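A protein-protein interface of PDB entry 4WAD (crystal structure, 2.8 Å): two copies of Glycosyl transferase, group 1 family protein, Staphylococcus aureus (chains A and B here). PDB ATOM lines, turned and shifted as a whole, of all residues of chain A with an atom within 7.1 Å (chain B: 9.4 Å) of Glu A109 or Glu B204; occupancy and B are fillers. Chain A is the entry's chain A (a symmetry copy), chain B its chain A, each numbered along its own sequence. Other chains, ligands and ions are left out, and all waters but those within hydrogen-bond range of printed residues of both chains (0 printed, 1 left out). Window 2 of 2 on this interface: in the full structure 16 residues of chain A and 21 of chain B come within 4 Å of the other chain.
Along chain A the printed residues that touch a printed residue of chain B span positions 107 to 117.
Hydrophobic or aromatic side chains of chain B that line the printed part of chain A: Tyr B197 and Leu B199.
Among the printed residues, 13 pairs touch across the chains.
Among the printed residues, Asp or Glu carboxylates within 4 Å of a Lys or Arg side-chain nitrogen of the other chain: Arg A115 with Glu B204.
The backbone carbonyl oxygen of Ser B183 sits at hydrogen-bond distance from the backbone NH of Tyr B197, 2.7 Å away.
N of Lys B195 sits at hydrogen-bond distance from O of Lys B206, at 3.3 Å.
O of Tyr B181 lies within hydrogen-bond range of N of Leu B199.
O of Lys B195 sits at hydrogen-bond distance from N of Asn B185 (2.9 Å).
O of Ile A107 sits at hydrogen-bond distance from N of Arg A115 (2.9 Å).
The backbone NH of Val B198 is in hydrogen-bond range of the backbone carbonyl oxygen of Lys B203, 2.7 Å away.
Among the printed residues, pairs that only touch across the chains: Phe A117 with Tyr B197 (3.4 Å), Glu A108 with Glu B204 (3.7 Å), Glu A109 with Glu B204 (3.7 Å), Phe A117 with Leu B199 (3.7 Å), Ile A107 with Glu B204 (3.7 Å), Arg A115 with Lys B195 (3.8 Å), Ile A107 with Leu B199 (3.8 Å), Ile A107 with Lys B202 (3.8 Å), Ile A107 with Tyr B197 (3.8 Å), Ile A107 with Lys B203 (3.9 Å) and Phe A117 with Ser B183 (3.96 Å).
The guanidinium group (NH2) of Arg A115 is in salt-bridge range of the side-chain carboxylate (OE2) of Glu B204 (3.7 Å).
The guanidinium group (NE) of Arg A115 lies close to the side-chain hydroxyl (OH) of Tyr B197, 3.4 Å away.
No position is printed for both chains.
Of the 13 pairs that touch across the chains among the printed residues, none has its exchanged pair printed and touching as well.
Glu A109 touches one residue of chain B.
Glu B204 touches just these residues of chain A: Ile A107, Glu A108, Glu A109 and Arg A115.
No residue of chain B comes within 4 Å of Ser A110.
Of the printed residues of chain A, Ser B183 touches Phe A117 (3.96 Å).
Printed residues of chain B within 4 Å of Ile A107: Tyr B197 (3.8 Å), Leu B199 (3.8 Å), Lys B202 (3.8 Å), Lys B203 (3.9 Å) and Glu B204 (3.7 Å).
Of the printed residues of chain A, Leu B199 touches Ile A107 (3.8 Å) and Phe A117 (3.7 Å).
Of the printed residues of chain A, Lys B202 touches Ile A107 (3.8 Å).
Printed residues of chain A within 4 Å of Tyr B197: Ile A107 (3.8 Å), Arg A115 (3.3 Å) and Phe A117 (3.4 Å).
Lys A111 touches none of the printed residues of chain B.
The nearest residue of chain A that does not touch Glu B204 is Ser A110 (5.8 Å).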
ATOM      1  N   ILE A 107     -15.811  22.867 -17.104  1.00  0.00           N
ATOM      2  CA  ILE A 107     -15.935  24.168 -16.459  1.00  0.00           C
ATOM      3  C   ILE A 107     -17.357  24.344 -15.945  1.00  0.00           C
ATOM      4  O   ILE A 107     -18.312  24.358 -16.726  1.00  0.00           O
ATOM      5  CB  ILE A 107     -15.578  25.318 -17.414  1.00  0.00           C
ATOM      6  CG1 ILE A 107     -14.115  25.218 -17.841  1.00  0.00           C
ATOM      7  CG2 ILE A 107     -15.842  26.661 -16.749  1.00  0.00           C
ATOM      8  CD1 ILE A 107     -13.654  26.368 -18.708  1.00  0.00           C
ATOM      9  N   GLU A 108     -17.493  24.475 -14.627  1.00  0.00           N
ATOM     10  CA  GLU A 108     -18.809  24.538 -13.997  1.00  0.00           C
ATOM     11  C   GLU A 108     -19.453  25.914 -14.113  1.00  0.00           C
ATOM     12  O   GLU A 108     -18.764  26.935 -14.158  1.00  0.00           O
ATOM     13  CB  GLU A 108     -18.708  24.139 -12.521  1.00  0.00           C
ATOM     14  CG  GLU A 108     -17.980  22.828 -12.278  1.00  0.00           C
ATOM     15  CD  GLU A 108     -17.905  22.472 -10.807  1.00  0.00           C
ATOM     16  OE1 GLU A 108     -18.556  23.165  -9.997  1.00  0.00           O
ATOM     17  OE2 GLU A 108     -17.200  21.498 -10.467  1.00  0.00           O
ATOM     18  N   GLU A 109     -20.783  25.925 -14.161  1.00  0.00           N
ATOM     19  CA  GLU A 109     -21.553  27.162 -14.111  1.00  0.00           C
ATOM     20  C   GLU A 109     -22.243  27.276 -12.754  1.00  0.00           C
ATOM     21  O   GLU A 109     -22.085  28.272 -12.046  1.00  0.00           O
ATOM     22  CB  GLU A 109     -22.583  27.206 -15.239  1.00  0.00           C
ATOM     23  CG  GLU A 109     -23.624  28.303 -15.091  1.00  0.00           C
ATOM     24  CD  GLU A 109     -24.644  28.281 -16.208  1.00  0.00           C
ATOM     25  OE1 GLU A 109     -25.855  28.225 -15.907  1.00  0.00           O
ATOM     26  OE2 GLU A 109     -24.229  28.320 -17.384  1.00  0.00           O
ATOM     27  N   SER A 110     -23.006  26.244 -12.406  1.00  0.00           N
ATOM     28  CA  SER A 110     -23.627  26.134 -11.091  1.00  0.00           C
ATOM     29  C   SER A 110     -23.542  24.690 -10.587  1.00  0.00           C
ATOM     30  O   SER A 110     -22.587  23.976 -10.901  1.00  0.00           O
ATOM     31  CB  SER A 110     -25.076  26.613 -11.138  1.00  0.00           C
ATOM     32  OG  SER A 110     -25.794  25.961 -12.161  1.00  0.00           O
ATOM     33  N   LYS A 111     -24.546  24.264  -9.822  1.00  0.00           N
ATOM     34  CA  LYS A 111     -24.534  22.951  -9.171  1.00  0.00           C
ATOM     35  C   LYS A 111     -24.425  21.783 -10.151  1.00  0.00           C
ATOM     36  O   LYS A 111     -23.437  21.049 -10.145  1.00  0.00           O
ATOM     37  CB  LYS A 111     -25.790  22.773  -8.314  1.00  0.00           C
ATOM     38  CG  LYS A 111     -25.830  21.450  -7.561  1.00  0.00           C
ATOM     39  CD  LYS A 111     -27.149  20.730  -7.788  1.00  0.00           C
ATOM     40  CE  LYS A 111     -26.919  19.239  -7.975  1.00  0.00           C
ATOM     41  NZ  LYS A 111     -28.073  18.569  -8.636  1.00  0.00           N
ATOM     42  N   GLY A 112     -25.446  21.606 -10.982  1.00  0.00           N
ATOM     43  CA  GLY A 112     -25.457  20.510 -11.936  1.00  0.00           C
ATOM     44  C   GLY A 112     -25.327  20.966 -13.377  1.00  0.00           C
ATOM     45  O   GLY A 112     -25.822  20.305 -14.291  1.00  0.00           O
ATOM     46  N   ILE A 113     -24.659  22.096 -13.580  1.00  0.00           N
ATOM     47  CA  ILE A 113     -24.483  22.656 -14.913  1.00  0.00           C
ATOM     48  C   ILE A 113     -23.002  22.841 -15.236  1.00  0.00           C
ATOM     49  O   ILE A 113     -22.280  23.512 -14.497  1.00  0.00           O
ATOM     50  CB  ILE A 113     -25.211  24.001 -15.046  1.00  0.00           C
ATOM     51  CG1 ILE A 113     -26.692  23.834 -14.700  1.00  0.00           C
ATOM     52  CG2 ILE A 113     -25.046  24.554 -16.445  1.00  0.00           C
ATOM     53  CD1 ILE A 113     -27.486  25.111 -14.804  1.00  0.00           C
ATOM     54  N   SER A 114     -22.553  22.243 -16.338  1.00  0.00           N
ATOM     55  CA  SER A 114     -21.148  22.314 -16.731  1.00  0.00           C
ATOM     56  C   SER A 114     -20.987  22.361 -18.245  1.00  0.00           C
ATOM     57  O   SER A 114     -21.815  21.824 -18.979  1.00  0.00           O
ATOM     58  CB  SER A 114     -20.375  21.117 -16.169  1.00  0.00           C
ATOM     59  OG  SER A 114     -20.495  21.048 -14.764  1.00  0.00           O
ATOM     60  N   ARG A 115     -19.919  23.009 -18.703  1.00  0.00           N
ATOM     61  CA  ARG A 115     -19.579  23.018 -20.121  1.00  0.00           C
ATOM     62  C   ARG A 115     -18.258  22.292 -20.329  1.00  0.00           C
ATOM     63  O   ARG A 115     -17.433  22.229 -19.417  1.00  0.00           O
ATOM     64  CB  ARG A 115     -19.508  24.453 -20.657  1.00  0.00           C
ATOM     65  CG  ARG A 115     -20.876  25.103 -20.806  1.00  0.00           C
ATOM     66  CD  ARG A 115     -20.787  26.561 -21.228  1.00  0.00           C
ATOM     67  NE  ARG A 115     -22.110  27.154 -21.410  1.00  0.00           N
ATOM     68  CZ  ARG A 115     -22.871  27.606 -20.416  1.00  0.00           C
ATOM     69  NH1 ARG A 115     -24.062  28.127 -20.674  1.00  0.00           N
ATOM     70  NH2 ARG A 115     -22.442  27.540 -19.164  1.00  0.00           N
ATOM     71  N   PHE A 117     -14.819  21.548 -22.900  1.00  0.00           N
ATOM     72  CA  PHE A 117     -13.996  22.088 -23.977  1.00  0.00           C
ATOM     73  C   PHE A 117     -12.863  21.133 -24.313  1.00  0.00           C
ATOM     74  O   PHE A 117     -12.214  20.600 -23.414  1.00  0.00           O
ATOM     75  CB  PHE A 117     -13.434  23.460 -23.587  1.00  0.00           C
ATOM     76  CG  PHE A 117     -14.486  24.487 -23.297  1.00  0.00           C
ATOM     77  CD1 PHE A 117     -14.997  24.639 -22.015  1.00  0.00           C
ATOM     78  CD2 PHE A 117     -14.969  25.299 -24.312  1.00  0.00           C
ATOM     79  CE1 PHE A 117     -15.974  25.587 -21.749  1.00  0.00           C
ATOM     80  CE2 PHE A 117     -15.946  26.248 -24.057  1.00  0.00           C
ATOM     81  CZ  PHE A 117     -16.448  26.392 -22.774  1.00  0.00           C
ATOM     82  N   TYR A 127     -22.644  21.011 -23.455  1.00  0.00           N
ATOM     83  CA  TYR A 127     -23.278  21.623 -22.293  1.00  0.00           C
ATOM     84  C   TYR A 127     -24.143  20.570 -21.613  1.00  0.00           C
ATOM     85  O   TYR A 127     -25.058  20.029 -22.234  1.00  0.00           O
ATOM     86  CB  TYR A 127     -24.117  22.837 -22.715  1.00  0.00           C
ATOM     87  CG  TYR A 127     -25.121  23.313 -21.688  1.00  0.00           C
ATOM     88  CD1 TYR A 127     -26.411  22.794 -21.649  1.00  0.00           C
ATOM     89  CD2 TYR A 127     -24.791  24.305 -20.781  1.00  0.00           C
ATOM     90  CE1 TYR A 127     -27.330  23.232 -20.723  1.00  0.00           C
ATOM     91  CE2 TYR A 127     -25.706  24.754 -19.852  1.00  0.00           C
ATOM     92  CZ  TYR A 127     -26.974  24.212 -19.828  1.00  0.00           C
ATOM     93  OH  TYR A 127     -27.891  24.652 -18.906  1.00  0.00           O
ATOM     94  N   ARG A 129     -26.668  19.744 -18.395  1.00  0.00           N
ATOM     95  CA  ARG A 129     -27.463  20.155 -17.246  1.00  0.00           C
ATOM     96  C   ARG A 129     -28.236  18.960 -16.719  1.00  0.00           C
ATOM     97  O   ARG A 129     -29.178  18.487 -17.363  1.00  0.00           O
ATOM     98  CB  ARG A 129     -28.421  21.288 -17.614  1.00  0.00           C
ATOM     99  CG  ARG A 129     -29.399  21.660 -16.504  1.00  0.00           C
ATOM    100  CD  ARG A 129     -30.250  22.845 -16.912  1.00  0.00           C
ATOM    101  NE  ARG A 129     -31.102  22.533 -18.056  1.00  0.00           N
ATOM    102  CZ  ARG A 129     -31.540  23.433 -18.930  1.00  0.00           C
ATOM    103  NH1 ARG A 129     -31.207  24.708 -18.792  1.00  0.00           N
ATOM    104  NH2 ARG A 129     -32.311  23.060 -19.942  1.00  0.00           N
ATOM    105  N   TYR B 181      -5.589  28.248 -23.460  1.00  0.00           N
ATOM    106  CA  TYR B 181      -5.721  28.716 -22.081  1.00  0.00           C
ATOM    107  C   TYR B 181      -6.976  29.564 -21.894  1.00  0.00           C
ATOM    108  O   TYR B 181      -7.535  29.621 -20.795  1.00  0.00           O
ATOM    109  CB  TYR B 181      -4.477  29.505 -21.650  1.00  0.00           C
ATOM    110  CG  TYR B 181      -4.144  30.706 -22.511  1.00  0.00           C
ATOM    111  CD1 TYR B 181      -3.306  30.581 -23.606  1.00  0.00           C
ATOM    112  CD2 TYR B 181      -4.643  31.966 -22.210  1.00  0.00           C
ATOM    113  CE1 TYR B 181      -2.989  31.666 -24.388  1.00  0.00           C
ATOM    114  CE2 TYR B 181      -4.331  33.060 -22.990  1.00  0.00           C
ATOM    115  CZ  TYR B 181      -3.503  32.903 -24.075  1.00  0.00           C
ATOM    116  OH  TYR B 181      -3.185  33.986 -24.858  1.00  0.00           O
ATOM    117  N   SER B 183     -10.743  30.764 -24.072  1.00  0.00           N
ATOM    118  CA  SER B 183     -11.670  30.816 -25.195  1.00  0.00           C
ATOM    119  C   SER B 183     -12.842  31.709 -24.821  1.00  0.00           C
ATOM    120  O   SER B 183     -13.149  31.856 -23.637  1.00  0.00           O
ATOM    121  CB  SER B 183     -12.159  29.423 -25.568  1.00  0.00           C
ATOM    122  OG  SER B 183     -13.128  28.969 -24.647  1.00  0.00           O
ATOM    123  N   ASN B 185     -16.823  33.673 -26.348  1.00  0.00           N
ATOM    124  CA  ASN B 185     -17.857  33.887 -27.352  1.00  0.00           C
ATOM    125  C   ASN B 185     -17.836  35.320 -27.872  1.00  0.00           C
ATOM    126  O   ASN B 185     -17.571  36.255 -27.115  1.00  0.00           O
ATOM    127  CB  ASN B 185     -19.236  33.554 -26.775  1.00  0.00           C
ATOM    128  CG  ASN B 185     -19.360  32.104 -26.364  1.00  0.00           C
ATOM    129  OD1 ASN B 185     -18.703  31.228 -26.927  1.00  0.00           O
ATOM    130  ND2 ASN B 185     -20.202  31.840 -25.368  1.00  0.00           N
ATOM    131  N   GLY B 194     -18.588  38.166 -25.192  1.00  0.00           N
ATOM    132  CA  GLY B 194     -19.508  37.594 -24.225  1.00  0.00           C
ATOM    133  C   GLY B 194     -18.800  36.683 -23.241  1.00  0.00           C
ATOM    134  O   GLY B 194     -17.740  37.033 -22.721  1.00  0.00           O
ATOM    135  N   LYS B 195     -19.387  35.515 -22.992  1.00  0.00           N
ATOM    136  CA  LYS B 195     -18.831  34.540 -22.056  1.00  0.00           C
ATOM    137  C   LYS B 195     -17.371  34.209 -22.350  1.00  0.00           C
ATOM    138  O   LYS B 195     -17.003  33.909 -23.489  1.00  0.00           O
ATOM    139  CB  LYS B 195     -19.667  33.262 -22.078  1.00  0.00           C
ATOM    140  CG  LYS B 195     -21.059  33.425 -21.512  1.00  0.00           C
ATOM    141  CD  LYS B 195     -21.098  33.030 -20.049  1.00  0.00           C
ATOM    142  CE  LYS B 195     -20.752  31.562 -19.875  1.00  0.00           C
ATOM    143  NZ  LYS B 195     -21.153  31.044 -18.540  1.00  0.00           N
ATOM    144  N   THR B 196     -16.549  34.274 -21.308  1.00  0.00           N
ATOM    145  CA  THR B 196     -15.117  34.020 -21.429  1.00  0.00           C
ATOM    146  C   THR B 196     -14.700  32.871 -20.512  1.00  0.00           C
ATOM    147  O   THR B 196     -14.877  32.944 -19.293  1.00  0.00           O
ATOM    148  CB  THR B 196     -14.299  35.281 -21.090  1.00  0.00           C
ATOM    149  OG1 THR B 196     -14.637  36.332 -22.005  1.00  0.00           O
ATOM    150  CG2 THR B 196     -12.806  34.995 -21.179  1.00  0.00           C
ATOM    151  N   TYR B 197     -14.145  31.817 -21.101  1.00  0.00           N
ATOM    152  CA  TYR B 197     -13.758  30.636 -20.340  1.00  0.00           C
ATOM    153  C   TYR B 197     -12.244  30.551 -20.183  1.00  0.00           C
ATOM    154  O   TYR B 197     -11.513  30.418 -21.171  1.00  0.00           O
ATOM    155  CB  TYR B 197     -14.299  29.369 -21.016  1.00  0.00           C
ATOM    156  CG  TYR B 197     -15.778  29.426 -21.325  1.00  0.00           C
ATOM    157  CD1 TYR B 197     -16.722  29.062 -20.374  1.00  0.00           C
ATOM    158  CD2 TYR B 197     -16.230  29.840 -22.569  1.00  0.00           C
ATOM    159  CE1 TYR B 197     -18.074  29.113 -20.655  1.00  0.00           C
ATOM    160  CE2 TYR B 197     -17.578  29.895 -22.857  1.00  0.00           C
ATOM    161  CZ  TYR B 197     -18.495  29.530 -21.897  1.00  0.00           C
ATOM    162  OH  TYR B 197     -19.837  29.583 -22.186  1.00  0.00           O
ATOM    163  N   VAL B 198     -11.776  30.645 -18.940  1.00  0.00           N
ATOM    164  CA  VAL B 198     -10.361  30.450 -18.645  1.00  0.00           C
ATOM    165  C   VAL B 198     -10.105  28.957 -18.469  1.00  0.00           C
ATOM    166  O   VAL B 198     -10.301  28.406 -17.383  1.00  0.00           O
ATOM    167  CB  VAL B 198      -9.921  31.227 -17.392  1.00  0.00           C
ATOM    168  CG1 VAL B 198      -8.423  31.066 -17.160  1.00  0.00           C
ATOM    169  CG2 VAL B 198     -10.264  32.693 -17.550  1.00  0.00           C
ATOM    170  N   LEU B 199      -9.677  28.314 -19.554  1.00  0.00           N
ATOM    171  CA  LEU B 199      -9.518  26.864 -19.604  1.00  0.00           C
ATOM    172  C   LEU B 199      -8.413  26.354 -18.675  1.00  0.00           C
ATOM    173  O   LEU B 199      -8.513  25.256 -18.122  1.00  0.00           O
ATOM    174  CB  LEU B 199      -9.233  26.425 -21.046  1.00  0.00           C
ATOM    175  CG  LEU B 199     -10.209  26.913 -22.122  1.00  0.00           C
ATOM    176  CD1 LEU B 199      -9.714  26.598 -23.525  1.00  0.00           C
ATOM    177  CD2 LEU B 199     -11.585  26.318 -21.907  1.00  0.00           C
ATOM    178  N   VAL B 200      -7.363  27.154 -18.504  1.00  0.00           N
ATOM    179  CA  VAL B 200      -6.205  26.744 -17.714  1.00  0.00           C
ATOM    180  C   VAL B 200      -6.544  26.667 -16.218  1.00  0.00           C
ATOM    181  O   VAL B 200      -5.952  25.878 -15.476  1.00  0.00           O
ATOM    182  CB  VAL B 200      -5.006  27.706 -17.950  1.00  0.00           C
ATOM    183  CG1 VAL B 200      -5.366  29.129 -17.557  1.00  0.00           C
ATOM    184  CG2 VAL B 200      -3.763  27.235 -17.208  1.00  0.00           C
ATOM    185  N   ASN B 201      -7.516  27.466 -15.783  1.00  0.00           N
ATOM    186  CA  ASN B 201      -7.948  27.434 -14.388  1.00  0.00           C
ATOM    187  C   ASN B 201      -9.371  26.900 -14.220  1.00  0.00           C
ATOM    188  O   ASN B 201      -9.925  26.938 -13.118  1.00  0.00           O
ATOM    189  CB  ASN B 201      -7.839  28.829 -13.765  1.00  0.00           C
ATOM    190  CG  ASN B 201      -6.399  29.286 -13.597  1.00  0.00           C
ATOM    191  OD1 ASN B 201      -5.478  28.471 -13.530  1.00  0.00           O
ATOM    192  ND2 ASN B 201      -6.199  30.597 -13.529  1.00  0.00           N
ATOM    193  N   LYS B 202      -9.949  26.408 -15.317  1.00  0.00           N
ATOM    194  CA  LYS B 202     -11.299  25.836 -15.319  1.00  0.00           C
ATOM    195  C   LYS B 202     -12.331  26.769 -14.695  1.00  0.00           C
ATOM    196  O   LYS B 202     -13.159  26.344 -13.888  1.00  0.00           O
ATOM    197  CB  LYS B 202     -11.315  24.489 -14.588  1.00  0.00           C
ATOM    198  CG  LYS B 202     -10.339  23.466 -15.152  1.00  0.00           C
ATOM    199  CD  LYS B 202     -10.480  22.127 -14.441  1.00  0.00           C
ATOM    200  CE  LYS B 202      -9.393  21.159 -14.878  1.00  0.00           C
ATOM    201  NZ  LYS B 202      -9.633  19.787 -14.354  1.00  0.00           N
ATOM    202  N   LYS B 203     -12.274  28.042 -15.075  1.00  0.00           N
ATOM    203  CA  LYS B 203     -13.184  29.044 -14.536  1.00  0.00           C
ATOM    204  C   LYS B 203     -13.860  29.799 -15.672  1.00  0.00           C
ATOM    205  O   LYS B 203     -13.251  30.030 -16.722  1.00  0.00           O
ATOM    206  CB  LYS B 203     -12.436  30.011 -13.614  1.00  0.00           C
ATOM    207  CG  LYS B 203     -13.340  30.831 -12.707  1.00  0.00           C
ATOM    208  CD  LYS B 203     -12.547  31.521 -11.606  1.00  0.00           C
ATOM    209  CE  LYS B 203     -13.471  32.232 -10.626  1.00  0.00           C
ATOM    210  NZ  LYS B 203     -14.886  31.794 -10.770  1.00  0.00           N
ATOM    211  N   GLU B 204     -15.120  30.170 -15.467  1.00  0.00           N
ATOM    212  CA  GLU B 204     -15.870  30.890 -16.488  1.00  0.00           C
ATOM    213  C   GLU B 204     -16.165  32.313 -16.035  1.00  0.00           C
ATOM    214  O   GLU B 204     -16.214  32.602 -14.837  1.00  0.00           O
ATOM    215  CB  GLU B 204     -17.175  30.164 -16.823  1.00  0.00           C
ATOM    216  CG  GLU B 204     -18.232  30.227 -15.730  1.00  0.00           C
ATOM    217  CD  GLU B 204     -19.603  29.820 -16.234  1.00  0.00           C
ATOM    218  OE1 GLU B 204     -20.613  30.323 -15.698  1.00  0.00           O
ATOM    219  OE2 GLU B 204     -19.671  28.997 -17.170  1.00  0.00           O
ATOM    220  N   PHE B 205     -16.352  33.205 -16.999  1.00  0.00           N
ATOM    221  CA  PHE B 205     -16.633  34.597 -16.693  1.00  0.00           C
ATOM    222  C   PHE B 205     -17.727  35.128 -17.609  1.00  0.00           C
ATOM    223  O   PHE B 205     -17.737  34.833 -18.805  1.00  0.00           O
ATOM    224  CB  PHE B 205     -15.354  35.434 -16.817  1.00  0.00           C
ATOM    225  CG  PHE B 205     -14.327  35.127 -15.761  1.00  0.00           C
ATOM    226  CD1 PHE B 205     -13.381  34.127 -15.956  1.00  0.00           C
ATOM    227  CD2 PHE B 205     -14.313  35.837 -14.568  1.00  0.00           C
ATOM    228  CE1 PHE B 205     -12.436  33.842 -14.979  1.00  0.00           C
ATOM    229  CE2 PHE B 205     -13.370  35.561 -13.586  1.00  0.00           C
ATOM    230  CZ  PHE B 205     -12.431  34.561 -13.794  1.00  0.00           C
ATOM    231  N   LYS B 206     -18.653  35.892 -17.031  1.00  0.00           N
ATOM    232  CA  LYS B 206     -19.786  36.458 -17.757  1.00  0.00           C
ATOM    233  C   LYS B 206     -19.349  37.218 -19.011  1.00  0.00           C
ATOM    234  O   LYS B 206     -19.904  37.021 -20.092  1.00  0.00           O
ATOM    235  CB  LYS B 206     -20.582  37.386 -16.836  1.00  0.00           C
ATOM    236  CG  LYS B 206     -21.662  38.194 -17.538  1.00  0.00           C
ATOM    237  CD  LYS B 206     -22.372  39.118 -16.566  1.00  0.00           C
ATOM    238  CE  LYS B 206     -23.434  39.938 -17.273  1.00  0.00           C
ATOM    239  NZ  LYS B 206     -24.160  40.837 -16.334  1.00  0.00           N
ATOM    240  N   ASN B 207     -18.343  38.076 -18.857  1.00  0.00           N
ATOM    241  CA  ASN B 207     -17.801  38.836 -19.980  1.00  0.00           C
ATOM    242  C   ASN B 207     -16.341  39.231 -19.761  1.00  0.00           C
ATOM    243  O   ASN B 207     -15.683  38.728 -18.850  1.00  0.00           O
ATOM    244  CB  ASN B 207     -18.650  40.084 -20.235  1.00  0.00           C
ATOM    245  CG  ASN B 207     -18.981  40.839 -18.959  1.00  0.00           C
ATOM    246  OD1 ASN B 207     -18.236  40.792 -17.980  1.00  0.00           O
ATOM    247  ND2 ASN B 207     -20.111  41.538 -18.965  1.00  0.00           N
ATOM    248  N   ASN B 208     -15.840  40.139 -20.594  1.00  0.00           N
ATOM    249  CA  ASN B 208     -14.465  40.609 -20.456  1.00  0.00           C
ATOM    250  C   ASN B 208     -14.295  41.483 -19.214  1.00  0.00           C
ATOM    251  O   ASN B 208     -13.219  41.523 -18.618  1.00  0.00           O
ATOM    252  CB  ASN B 208     -14.029  41.376 -21.711  1.00  0.00           C
ATOM    253  CG  ASN B 208     -12.520  41.539 -21.807  1.00  0.00           C
ATOM    254  OD1 ASN B 208     -11.763  40.641 -21.437  1.00  0.00           O
ATOM    255  ND2 ASN B 208     -12.077  42.686 -22.309  1.00  0.00           N
ATOM    256  N   ALA B 210     -15.861  41.121 -16.247  1.00  0.00           N
ATOM    257  CA  ALA B 210     -15.717  40.228 -15.106  1.00  0.00           C
ATOM    258  C   ALA B 210     -14.350  39.546 -15.090  1.00  0.00           C
ATOM    259  O   ALA B 210     -13.853  39.167 -14.030  1.00  0.00           O
ATOM    260  CB  ALA B 210     -16.822  39.186 -15.114  1.00  0.00           C
ATOM    261  N   LEU B 211     -13.753  39.384 -16.270  1.00  0.00           N
ATOM    262  CA  LEU B 211     -12.454  38.724 -16.395  1.00  0.00           C
ATOM    263  C   LEU B 211     -11.312  39.628 -15.952  1.00  0.00           C
ATOM    264  O   LEU B 211     -10.400  39.185 -15.255  1.00  0.00           O
ATOM    265  CB  LEU B 211     -12.218  38.266 -17.839  1.00  0.00           C
ATOM    266  CG  LEU B 211     -10.816  37.731 -18.136  1.00  0.00           C
ATOM    267  CD1 LEU B 211     -10.590  36.415 -17.418  1.00  0.00           C
ATOM    268  CD2 LEU B 211     -10.582  37.566 -19.629  1.00  0.00           C
ATOM    269  N   TYR B 214     -11.284  40.324 -12.093  1.00  0.00           N
ATOM    270  CA  TYR B 214     -10.614  39.185 -11.476  1.00  0.00           C
ATOM    271  C   TYR B 214      -9.110  39.251 -11.694  1.00  0.00           C
ATOM    272  O   TYR B 214      -8.333  38.890 -10.813  1.00  0.00           O
ATOM    273  CB  TYR B 214     -11.173  37.873 -12.038  1.00  0.00           C
ATOM    274  CG  TYR B 214     -10.403  36.633 -11.635  1.00  0.00           C
ATOM    275  CD1 TYR B 214     -10.674  35.982 -10.441  1.00  0.00           C
ATOM    276  CD2 TYR B 214      -9.419  36.102 -12.461  1.00  0.00           C
ATOM    277  CE1 TYR B 214      -9.977  34.845 -10.072  1.00  0.00           C
ATOM    278  CE2 TYR B 214      -8.716  34.968 -12.100  1.00  0.00           C
ATOM    279  CZ  TYR B 214      -9.001  34.344 -10.904  1.00  0.00           C
ATOM    280  OH  TYR B 214      -8.307  33.215 -10.543  1.00  0.00           O
